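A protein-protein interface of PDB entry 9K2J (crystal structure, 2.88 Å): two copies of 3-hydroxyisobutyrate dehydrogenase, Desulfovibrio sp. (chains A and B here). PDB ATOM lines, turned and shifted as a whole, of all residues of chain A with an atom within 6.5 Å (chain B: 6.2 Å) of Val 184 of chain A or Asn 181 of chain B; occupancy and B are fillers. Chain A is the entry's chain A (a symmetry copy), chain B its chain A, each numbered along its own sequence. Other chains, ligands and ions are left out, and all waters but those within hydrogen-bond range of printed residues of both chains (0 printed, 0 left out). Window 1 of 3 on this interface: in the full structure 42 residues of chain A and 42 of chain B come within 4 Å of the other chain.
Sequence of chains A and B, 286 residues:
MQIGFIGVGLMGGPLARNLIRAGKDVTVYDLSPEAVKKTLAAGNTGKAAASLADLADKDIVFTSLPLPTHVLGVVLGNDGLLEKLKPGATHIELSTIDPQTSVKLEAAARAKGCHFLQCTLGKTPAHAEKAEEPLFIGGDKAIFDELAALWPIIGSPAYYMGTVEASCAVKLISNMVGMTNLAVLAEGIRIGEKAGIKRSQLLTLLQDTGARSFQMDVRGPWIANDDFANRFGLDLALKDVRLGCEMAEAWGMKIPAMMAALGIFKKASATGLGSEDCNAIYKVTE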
ATOM      1  N   VAL A 177      -7.395 -20.297  -9.463  1.00  0.00           N
ATOM      2  CA  VAL A 177      -6.038 -19.773  -9.371  1.00  0.00           C
ATOM      3  C   VAL A 177      -5.315 -20.363  -8.166  1.00  0.00           C
ATOM      4  O   VAL A 177      -4.144 -20.744  -8.273  1.00  0.00           O
ATOM      5  CB  VAL A 177      -6.055 -18.230  -9.335  1.00  0.00           C
ATOM      6  CG1 VAL A 177      -4.688 -17.710  -9.061  1.00  0.00           C
ATOM      7  CG2 VAL A 177      -6.533 -17.673 -10.641  1.00  0.00           C
ATOM      8  N   MET A 179      -5.853 -23.245  -6.557  1.00  0.00           N
ATOM      9  CA  MET A 179      -5.572 -24.668  -6.689  1.00  0.00           C
ATOM     10  C   MET A 179      -4.577 -24.940  -7.803  1.00  0.00           C
ATOM     11  O   MET A 179      -3.756 -25.854  -7.677  1.00  0.00           O
ATOM     12  CB  MET A 179      -6.886 -25.429  -6.878  1.00  0.00           C
ATOM     13  CG  MET A 179      -7.775 -25.232  -5.677  1.00  0.00           C
ATOM     14  SD  MET A 179      -6.978 -25.822  -4.150  1.00  0.00           S
ATOM     15  CE  MET A 179      -6.392 -24.331  -3.349  1.00  0.00           C
ATOM     16  N   THR A 180      -4.591 -24.134  -8.871  1.00  0.00           N
ATOM     17  CA  THR A 180      -3.544 -24.256  -9.878  1.00  0.00           C
ATOM     18  C   THR A 180      -2.195 -23.812  -9.329  1.00  0.00           C
ATOM     19  O   THR A 180      -1.169 -24.437  -9.616  1.00  0.00           O
ATOM     20  CB  THR A 180      -3.908 -23.464 -11.125  1.00  0.00           C
ATOM     21  OG1 THR A 180      -5.234 -23.824 -11.530  1.00  0.00           O
ATOM     22  CG2 THR A 180      -2.978 -23.832 -12.230  1.00  0.00           C
ATOM     23  N   ASN A 181      -2.167 -22.731  -8.555  1.00  0.00           N
ATOM     24  CA  ASN A 181      -0.942 -22.366  -7.867  1.00  0.00           C
ATOM     25  C   ASN A 181      -0.417 -23.545  -7.064  1.00  0.00           C
ATOM     26  O   ASN A 181       0.780 -23.844  -7.102  1.00  0.00           O
ATOM     27  CB  ASN A 181      -1.191 -21.162  -6.966  1.00  0.00           C
ATOM     28  CG  ASN A 181      -1.165 -19.845  -7.723  1.00  0.00           C
ATOM     29  OD1 ASN A 181      -1.219 -19.811  -8.958  1.00  0.00           O
ATOM     30  ND2 ASN A 181      -1.086 -18.743  -6.978  1.00  0.00           N
ATOM     31  N   LEU A 182      -1.311 -24.251  -6.354  1.00  0.00           N
ATOM     32  CA  LEU A 182      -0.882 -25.404  -5.561  1.00  0.00           C
ATOM     33  C   LEU A 182      -0.368 -26.544  -6.440  1.00  0.00           C
ATOM     34  O   LEU A 182       0.678 -27.129  -6.145  1.00  0.00           O
ATOM     35  CB  LEU A 182      -2.022 -25.903  -4.685  1.00  0.00           C
ATOM     36  CG  LEU A 182      -1.544 -27.026  -3.766  1.00  0.00           C
ATOM     37  CD1 LEU A 182      -0.432 -26.550  -2.848  1.00  0.00           C
ATOM     38  CD2 LEU A 182      -2.667 -27.551  -2.955  1.00  0.00           C
ATOM     39  N   ALA A 183      -1.075 -26.871  -7.523  1.00  0.00           N
ATOM     40  CA  ALA A 183      -0.607 -27.928  -8.422  1.00  0.00           C
ATOM     41  C   ALA A 183       0.763 -27.588  -9.015  1.00  0.00           C
ATOM     42  O   ALA A 183       1.631 -28.462  -9.154  1.00  0.00           O
ATOM     43  CB  ALA A 183      -1.643 -28.171  -9.526  1.00  0.00           C
ATOM     44  N   VAL A 184       0.980 -26.317  -9.358  1.00  0.00           N
ATOM     45  CA  VAL A 184       2.253 -25.868  -9.913  1.00  0.00           C
ATOM     46  C   VAL A 184       3.361 -25.936  -8.862  1.00  0.00           C
ATOM     47  O   VAL A 184       4.500 -26.326  -9.157  1.00  0.00           O
ATOM     48  CB  VAL A 184       2.065 -24.449 -10.470  1.00  0.00           C
ATOM     49  CG1 VAL A 184       3.400 -23.807 -10.818  1.00  0.00           C
ATOM     50  CG2 VAL A 184       1.098 -24.502 -11.666  1.00  0.00           C
ATOM     51  N   LEU A 185       3.044 -25.548  -7.623  1.00  0.00           N
ATOM     52  CA  LEU A 185       3.984 -25.697  -6.516  1.00  0.00           C
ATOM     53  C   LEU A 185       4.371 -27.159  -6.312  1.00  0.00           C
ATOM     54  O   LEU A 185       5.541 -27.480  -6.061  1.00  0.00           O
ATOM     55  CB  LEU A 185       3.358 -25.121  -5.241  1.00  0.00           C
ATOM     56  CG  LEU A 185       4.012 -25.422  -3.900  1.00  0.00           C
ATOM     57  CD1 LEU A 185       5.298 -24.623  -3.712  1.00  0.00           C
ATOM     58  CD2 LEU A 185       3.038 -25.100  -2.806  1.00  0.00           C
ATOM     59  N   ALA A 186       3.391 -28.057  -6.390  1.00  0.00           N
ATOM     60  CA  ALA A 186       3.683 -29.479  -6.290  1.00  0.00           C
ATOM     61  C   ALA A 186       4.624 -29.917  -7.405  1.00  0.00           C
ATOM     62  O   ALA A 186       5.564 -30.686  -7.170  1.00  0.00           O
ATOM     63  CB  ALA A 186       2.379 -30.280  -6.317  1.00  0.00           C
ATOM     64  N   GLU A 187       4.368 -29.454  -8.635  1.00  0.00           N
ATOM     65  CA  GLU A 187       5.269 -29.770  -9.739  1.00  0.00           C
ATOM     66  C   GLU A 187       6.689 -29.290  -9.438  1.00  0.00           C
ATOM     67  O   GLU A 187       7.663 -30.032  -9.629  1.00  0.00           O
ATOM     68  CB  GLU A 187       4.738 -29.157 -11.038  1.00  0.00           C
ATOM     69  CG  GLU A 187       3.526 -29.911 -11.610  1.00  0.00           C
ATOM     70  CD  GLU A 187       3.009 -29.372 -12.969  1.00  0.00           C
ATOM     71  OE1 GLU A 187       3.583 -28.405 -13.521  1.00  0.00           O
ATOM     72  OE2 GLU A 187       2.037 -29.951 -13.511  1.00  0.00           O
ATOM     73  N   GLY A 188       6.822 -28.073  -8.905  1.00  0.00           N
ATOM     74  CA  GLY A 188       8.146 -27.561  -8.578  1.00  0.00           C
ATOM     75  C   GLY A 188       8.855 -28.385  -7.517  1.00  0.00           C
ATOM     76  O   GLY A 188      10.055 -28.658  -7.629  1.00  0.00           O
ATOM     77  N   ILE A 189       8.128 -28.765  -6.456  1.00  0.00           N
ATOM     78  CA  ILE A 189       8.711 -29.529  -5.351  1.00  0.00           C
ATOM     79  C   ILE A 189       9.160 -30.895  -5.842  1.00  0.00           C
ATOM     80  O   ILE A 189      10.244 -31.390  -5.495  1.00  0.00           O
ATOM     81  CB  ILE A 189       7.686 -29.661  -4.208  1.00  0.00           C
ATOM     82  CG1 ILE A 189       7.594 -28.380  -3.397  1.00  0.00           C
ATOM     83  CG2 ILE A 189       8.041 -30.827  -3.290  1.00  0.00           C
ATOM     84  CD1 ILE A 189       6.552 -28.453  -2.352  1.00  0.00           C
ATOM     85  N   GLY A 210      10.569 -14.954  -6.955  1.00  0.00           N
ATOM     86  CA  GLY A 210       9.343 -14.634  -7.654  1.00  0.00           C
ATOM     87  C   GLY A 210       8.385 -15.785  -7.798  1.00  0.00           C
ATOM     88  O   GLY A 210       7.336 -15.643  -8.436  1.00  0.00           O
ATOM     89  N   ALA A 211       8.729 -16.934  -7.240  1.00  0.00           N
ATOM     90  CA  ALA A 211       7.864 -18.098  -7.249  1.00  0.00           C
ATOM     91  C   ALA A 211       6.953 -18.134  -6.030  1.00  0.00           C
ATOM     92  O   ALA A 211       6.109 -19.038  -5.910  1.00  0.00           O
ATOM     93  CB  ALA A 211       8.717 -19.360  -7.324  1.00  0.00           C
ATOM     94  N   ARG A 212       7.131 -17.186  -5.116  1.00  0.00           N
ATOM     95  CA  ARG A 212       6.404 -17.209  -3.859  1.00  0.00           C
ATOM     96  C   ARG A 212       4.906 -17.099  -4.129  1.00  0.00           C
ATOM     97  O   ARG A 212       4.474 -16.429  -5.072  1.00  0.00           O
ATOM     98  CB  ARG A 212       6.831 -16.045  -2.976  1.00  0.00           C
ATOM     99  CG  ARG A 212       6.533 -16.298  -1.540  1.00  0.00           C
ATOM    100  CD  ARG A 212       6.832 -15.132  -0.632  1.00  0.00           C
ATOM    101  NE  ARG A 212       6.963 -15.631   0.733  1.00  0.00           N
ATOM    102  CZ  ARG A 212       7.067 -14.894   1.828  1.00  0.00           C
ATOM    103  NH1 ARG A 212       6.941 -13.574   1.768  1.00  0.00           N
ATOM    104  NH2 ARG A 212       7.269 -15.486   2.994  1.00  0.00           N
ATOM    105  N   SER A 213       4.112 -17.795  -3.326  1.00  0.00           N
ATOM    106  CA  SER A 213       2.665 -17.672  -3.405  1.00  0.00           C
ATOM    107  C   SER A 213       2.081 -17.991  -2.039  1.00  0.00           C
ATOM    108  O   SER A 213       2.749 -18.564  -1.173  1.00  0.00           O
ATOM    109  CB  SER A 213       2.072 -18.575  -4.497  1.00  0.00           C
ATOM    110  OG  SER A 213       2.550 -19.899  -4.374  1.00  0.00           O
ATOM    111  N   ALA A 257      -3.310 -24.213 -18.472  1.00  0.00           N
ATOM    112  CA  ALA A 257      -2.662 -24.550 -17.212  1.00  0.00           C
ATOM    113  C   ALA A 257      -3.692 -25.000 -16.185  1.00  0.00           C
ATOM    114  O   ALA A 257      -3.505 -26.025 -15.505  1.00  0.00           O
ATOM    115  CB  ALA A 257      -1.850 -23.356 -16.701  1.00  0.00           C
ATOM    116  N   ALA A 261      -4.253 -28.532 -14.071  1.00  0.00           N
ATOM    117  CA  ALA A 261      -4.558 -28.634 -12.643  1.00  0.00           C
ATOM    118  C   ALA A 261      -5.815 -29.473 -12.413  1.00  0.00           C
ATOM    119  O   ALA A 261      -5.854 -30.344 -11.528  1.00  0.00           O
ATOM    120  CB  ALA A 261      -4.719 -27.235 -12.026  1.00  0.00           C
ATOM    121  N   ILE A 281      -2.602 -33.651  -3.792  1.00  0.00           N
ATOM    122  CA  ILE A 281      -2.292 -33.841  -5.219  1.00  0.00           C
ATOM    123  C   ILE A 281      -0.790 -34.008  -5.429  1.00  0.00           C
ATOM    124  O   ILE A 281      -0.352 -34.634  -6.408  1.00  0.00           O
ATOM    125  CB  ILE A 281      -2.834 -32.686  -6.080  1.00  0.00           C
ATOM    126  CG1 ILE A 281      -2.206 -31.366  -5.650  1.00  0.00           C
ATOM    127  CG2 ILE A 281      -4.333 -32.621  -5.989  1.00  0.00           C
ATOM    128  CD1 ILE A 281      -2.644 -30.223  -6.494  1.00  0.00           C
ATOM    129  N   MET B 176      10.481 -21.520 -13.474  1.00  0.00           N
ATOM    130  CA  MET B 176       9.336 -22.314 -13.939  1.00  0.00           C
ATOM    131  C   MET B 176       8.091 -22.016 -13.107  1.00  0.00           C
ATOM    132  O   MET B 176       7.011 -21.730 -13.646  1.00  0.00           O
ATOM    133  CB  MET B 176       9.670 -23.807 -13.879  1.00  0.00           C
ATOM    134  CG  MET B 176      10.756 -24.218 -14.851  1.00  0.00           C
ATOM    135  SD  MET B 176      11.337 -25.903 -14.633  1.00  0.00           S
ATOM    136  CE  MET B 176       9.972 -26.810 -15.309  1.00  0.00           C
ATOM    137  N   VAL B 177       8.237 -22.043 -11.781  1.00  0.00           N
ATOM    138  CA  VAL B 177       7.113 -21.785 -10.890  1.00  0.00           C
ATOM    139  C   VAL B 177       6.646 -20.340 -11.019  1.00  0.00           C
ATOM    140  O   VAL B 177       5.438 -20.084 -11.068  1.00  0.00           O
ATOM    141  CB  VAL B 177       7.484 -22.144  -9.435  1.00  0.00           C
ATOM    142  CG1 VAL B 177       6.401 -21.711  -8.511  1.00  0.00           C
ATOM    143  CG2 VAL B 177       7.688 -23.621  -9.287  1.00  0.00           C
ATOM    144  N   GLY B 178       7.582 -19.374 -11.073  1.00  0.00           N
ATOM    145  CA  GLY B 178       7.173 -17.986 -11.171  1.00  0.00           C
ATOM    146  C   GLY B 178       6.445 -17.692 -12.470  1.00  0.00           C
ATOM    147  O   GLY B 178       5.410 -17.014 -12.481  1.00  0.00           O
ATOM    148  N   MET B 179       6.957 -18.219 -13.585  1.00  0.00           N
ATOM    149  CA  MET B 179       6.340 -17.922 -14.871  1.00  0.00           C
ATOM    150  C   MET B 179       5.037 -18.681 -15.054  1.00  0.00           C
ATOM    151  O   MET B 179       4.102 -18.148 -15.660  1.00  0.00           O
ATOM    152  CB  MET B 179       7.344 -18.202 -15.992  1.00  0.00           C
ATOM    153  CG  MET B 179       8.554 -17.318 -15.834  1.00  0.00           C
ATOM    154  SD  MET B 179       8.108 -15.555 -15.882  1.00  0.00           S
ATOM    155  CE  MET B 179       8.119 -15.045 -14.165  1.00  0.00           C
ATOM    156  N   THR B 180       4.930 -19.892 -14.497  1.00  0.00           N
ATOM    157  CA  THR B 180       3.643 -20.576 -14.505  1.00  0.00           C
ATOM    158  C   THR B 180       2.637 -19.870 -13.605  1.00  0.00           C
ATOM    159  O   THR B 180       1.459 -19.754 -13.959  1.00  0.00           O
ATOM    160  CB  THR B 180       3.809 -22.031 -14.093  1.00  0.00           C
ATOM    161  OG1 THR B 180       4.853 -22.617 -14.879  1.00  0.00           O
ATOM    162  CG2 THR B 180       2.548 -22.771 -14.382  1.00  0.00           C
ATOM    163  N   ASN B 181       3.070 -19.407 -12.436  1.00  0.00           N
ATOM    164  CA  ASN B 181       2.201 -18.578 -11.621  1.00  0.00           C
ATOM    165  C   ASN B 181       1.674 -17.407 -12.435  1.00  0.00           C
ATOM    166  O   ASN B 181       0.478 -17.101 -12.387  1.00  0.00           O
ATOM    167  CB  ASN B 181       2.955 -18.088 -10.390  1.00  0.00           C
ATOM    168  CG  ASN B 181       3.012 -19.128  -9.283  1.00  0.00           C
ATOM    169  OD1 ASN B 181       2.723 -20.312  -9.495  1.00  0.00           O
ATOM    170  ND2 ASN B 181       3.394 -18.686  -8.085  1.00  0.00           N
ATOM    171  N   LEU B 182       2.549 -16.761 -13.219  1.00  0.00           N
ATOM    172  CA  LEU B 182       2.114 -15.627 -14.038  1.00  0.00           C
ATOM    173  C   LEU B 182       1.133 -16.054 -15.129  1.00  0.00           C
ATOM    174  O   LEU B 182       0.109 -15.394 -15.332  1.00  0.00           O
ATOM    175  CB  LEU B 182       3.314 -14.931 -14.666  1.00  0.00           C
ATOM    176  CG  LEU B 182       2.875 -13.677 -15.419  1.00  0.00           C
ATOM    177  CD1 LEU B 182       2.201 -12.684 -14.487  1.00  0.00           C
ATOM    178  CD2 LEU B 182       4.034 -13.031 -16.078  1.00  0.00           C
ATOM    179  N   ALA B 183       1.416 -17.149 -15.837  1.00  0.00           N
ATOM    180  CA  ALA B 183       0.491 -17.624 -16.867  1.00  0.00           C
ATOM    181  C   ALA B 183      -0.879 -17.963 -16.272  1.00  0.00           C
ATOM    182  O   ALA B 183      -1.923 -17.680 -16.877  1.00  0.00           O
ATOM    183  CB  ALA B 183       1.094 -18.834 -17.591  1.00  0.00           C
ATOM    184  N   VAL B 184      -0.894 -18.557 -15.078  1.00  0.00           N
ATOM    185  CA  VAL B 184      -2.138 -18.909 -14.400  1.00  0.00           C
ATOM    186  C   VAL B 184      -2.892 -17.655 -13.958  1.00  0.00           C
ATOM    187  O   VAL B 184      -4.125 -17.580 -14.060  1.00  0.00           O
ATOM    188  CB  VAL B 184      -1.802 -19.833 -13.220  1.00  0.00           C
ATOM    189  CG1 VAL B 184      -3.003 -20.024 -12.305  1.00  0.00           C
ATOM    190  CG2 VAL B 184      -1.248 -21.162 -13.764  1.00  0.00           C
ATOM    191  N   LEU B 185      -2.162 -16.657 -13.453  1.00  0.00           N
ATOM    192  CA  LEU B 185      -2.761 -15.367 -13.123  1.00  0.00           C
ATOM    193  C   LEU B 185      -3.392 -14.720 -14.354  1.00  0.00           C
ATOM    194  O   LEU B 185      -4.485 -14.142 -14.281  1.00  0.00           O
ATOM    195  CB  LEU B 185      -1.690 -14.452 -12.520  1.00  0.00           C
ATOM    196  CG  LEU B 185      -1.990 -12.967 -12.372  1.00  0.00           C
ATOM    197  CD1 LEU B 185      -2.960 -12.705 -11.223  1.00  0.00           C
ATOM    198  CD2 LEU B 185      -0.703 -12.236 -12.139  1.00  0.00           C
ATOM    199  N   ALA B 186      -2.699 -14.786 -15.488  1.00  0.00           N
ATOM    200  CA  ALA B 186      -3.260 -14.268 -16.728  1.00  0.00           C
ATOM    201  C   ALA B 186      -4.550 -14.998 -17.082  1.00  0.00           C
ATOM    202  O   ALA B 186      -5.534 -14.374 -17.499  1.00  0.00           O
ATOM    203  CB  ALA B 186      -2.230 -14.384 -17.853  1.00  0.00           C
ATOM    204  N   SER B 213      -0.221 -14.326  -5.055  1.00  0.00           N
ATOM    205  CA  SER B 213       1.135 -14.754  -5.360  1.00  0.00           C
ATOM    206  C   SER B 213       1.992 -13.518  -5.572  1.00  0.00           C
ATOM    207  O   SER B 213       1.484 -12.409  -5.763  1.00  0.00           O
ATOM    208  CB  SER B 213       1.180 -15.687  -6.580  1.00  0.00           C
ATOM    209  OG  SER B 213       0.473 -15.131  -7.669  1.00  0.00           O
ATOM    210  N   PHE B 214       3.310 -13.723  -5.506  1.00  0.00           N
ATOM    211  CA  PHE B 214       4.245 -12.642  -5.798  1.00  0.00           C
ATOM    212  C   PHE B 214       3.976 -12.045  -7.176  1.00  0.00           C
ATOM    213  O   PHE B 214       3.940 -10.823  -7.333  1.00  0.00           O
ATOM    214  CB  PHE B 214       5.674 -13.170  -5.672  1.00  0.00           C
ATOM    215  CG  PHE B 214       6.745 -12.201  -6.124  1.00  0.00           C
ATOM    216  CD1 PHE B 214       7.203 -12.204  -7.424  1.00  0.00           C
ATOM    217  CD2 PHE B 214       7.305 -11.299  -5.228  1.00  0.00           C
ATOM    218  CE1 PHE B 214       8.197 -11.334  -7.811  1.00  0.00           C
ATOM    219  CE2 PHE B 214       8.292 -10.427  -5.610  1.00  0.00           C
ATOM    220  CZ  PHE B 214       8.734 -10.438  -6.899  1.00  0.00           C
ATOM    221  N   GLN B 215       3.725 -12.889  -8.176  1.00  0.00           N
ATOM    222  CA  GLN B 215       3.444 -12.344  -9.493  1.00  0.00           C
ATOM    223  C   GLN B 215       2.163 -11.538  -9.469  1.00  0.00           C
ATOM    224  O   GLN B 215       2.086 -10.496 -10.119  1.00  0.00           O
ATOM    225  CB  GLN B 215       3.348 -13.443 -10.546  1.00  0.00           C
ATOM    226  CG  GLN B 215       4.599 -14.250 -10.661  1.00  0.00           C
ATOM    227  CD  GLN B 215       5.745 -13.419 -11.170  1.00  0.00           C
ATOM    228  OE1 GLN B 215       5.616 -12.750 -12.186  1.00  0.00           O
ATOM    229  NE2 GLN B 215       6.863 -13.420 -10.441  1.00  0.00           N
ATOM    230  N   ALA B 257       1.020 -28.627 -15.992  1.00  0.00           N
ATOM    231  CA  ALA B 257       0.694 -27.211 -15.893  1.00  0.00           C
ATOM    232  C   ALA B 257       1.844 -26.361 -16.416  1.00  0.00           C
ATOM    233  O   ALA B 257       1.631 -25.421 -17.202  1.00  0.00           O
ATOM    234  CB  ALA B 257       0.346 -26.850 -14.446  1.00  0.00           C
ATOM    235  N   MET B 258       3.078 -26.716 -16.032  1.00  0.00           N
ATOM    236  CA  MET B 258       4.250 -25.994 -16.517  1.00  0.00           C
ATOM    237  C   MET B 258       4.416 -26.162 -18.020  1.00  0.00           C
ATOM    238  O   MET B 258       4.804 -25.219 -18.708  1.00  0.00           O
ATOM    239  CB  MET B 258       5.491 -26.455 -15.762  1.00  0.00           C
ATOM    240  CG  MET B 258       5.417 -26.092 -14.300  1.00  0.00           C
ATOM    241  SD  MET B 258       6.798 -26.629 -13.268  1.00  0.00           S
ATOM    242  CE  MET B 258       6.796 -25.307 -12.080  1.00  0.00           C
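The backbone NH (N) of Ala 257 of chain B lies within hydrogen-bond range of the side-chain carboxylate (OE2) of Glu 187 of chain A (3.0 Å). OE1 of Glu 187 of chain A lies close to N of Met 258 of chain B (3.1 Å). The backbone carbonyl oxygen (O) of Arg 212 of chain A lies within hydrogen-bond range of the backbone NH (N) of Phe 214 of chain B, at 3.0 Å. The side-chain amide nitrogen of Gln 215 of chain B is in hydrogen-bond range of the backbone carbonyl oxygen of Gly 210 of chain A (3.0 Å). ND2 of Asn 181 of chain B lies within hydrogen-bond range of O of Ala 211 of chain A (3.5 Å).
OD1 of Asn 181 of chain B lies close to O of Val 177 of chain B (3.1 Å). The backbone carbonyl oxygen of Val 177 of chain A sits close to the side-chain amide oxygen of Asn 181 of chain A (3.1 Å). O of Met 176 of chain B is in hydrogen-bond range of OG1 of Thr 180 of chain B, 2.6 Å away.
Val 184 of chain B touches Thr 180 of chain A (CG2 to CG2, 3.5 Å). OD1 of Asn 181 of chain A touches CG1 of Val 184 of chain B, at 3.8 Å. ND2 of Asn 181 of chain A touches CB of Ser 213 of chain B, 3.8 Å away. Val 184 of chain A touches Ala 257 of chain B (CG2 to CB, 3.7 Å). CA of Gly 210 of chain A touches CD1 of Phe 214 of chain B, at 3.2 Å. CB of Ala 211 of chain A touches CG1 of Val 177 of chain B (3.5 Å). CB of Ala 211 of chain A touches N of Gly 178 of chain B (3.9 Å). Arg 212 of chain A touches Ser 213 of chain B (O to CB, 3.7 Å). Ser 213 of chain A touches Ser 213 of chain B. Val 184 of chain B touches Ala 257 of chain A (CG2 to CB, 3.7 Å).
Printed residues of chain B within 4 Å of Asn 181 of chain A: Val 184 (3.8 Å) and Ser 213 (3.8 Å). Printed residues of chain B within 4 Å of Val 184 of chain A: Thr 180, Asn 181, Ala 257 and Met 258. Ile 189 of chain A touches none of the printed residues of chain B. Of the printed residues of chain A, Asn 181 of chain B touches Val 184 (3.8 Å), Ala 211 (3.5 Å), Arg 212 (3.9 Å) and Ser 213 (3.8 Å). Printed residues of chain A within 4 Å of Ser 213 of chain B: Asn 181, Arg 212 and Ser 213. The nearest printed residue of chain A that does not touch Asn 181 of chain B is Asn 181 of chain A (4.01 Å). The nearest printed residue of chain A that does not touch Ala 257 of chain B is Ala 257 of chain A (4.1 Å).
Along chain B the printed residues that touch a printed residue of chain A span positions 177 to 258. Hydrophobic or aromatic side chains of chain A within 4 Å of the printed part of chain B: Val 184, Ala 211 and Ala 257. Among the printed residues, 21 pairs touch across the chains. Among the printed residues, no Asp or Glu carboxylate lies within 4 Å of a Lys or Arg side-chain nitrogen of the other chain.
Thr 180 of chain A touches Val 184 of chain B, and with the chains exchanged Val 184 of chain A touches Thr 180 of chain B. Asn 181 of chain A touches Val 184 of chain B, and with the chains exchanged Val 184 of chain A touches Asn 181 of chain B. Val 184 of chain A touches Ala 257 of chain B, and with the chains exchanged Ala 257 of chain A touches Val 184 of chain B. Ser 213 of chain B touches its own counterpart, Ser 213 of chain A. Positions printed for both chains: 177, 179, 180, 181, 182, 183, 184, 185, 186, 213 and 257. Of the 21 pairs that touch across the chains among the printed residues, 9 have their exchanged pair printed and touching as well.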
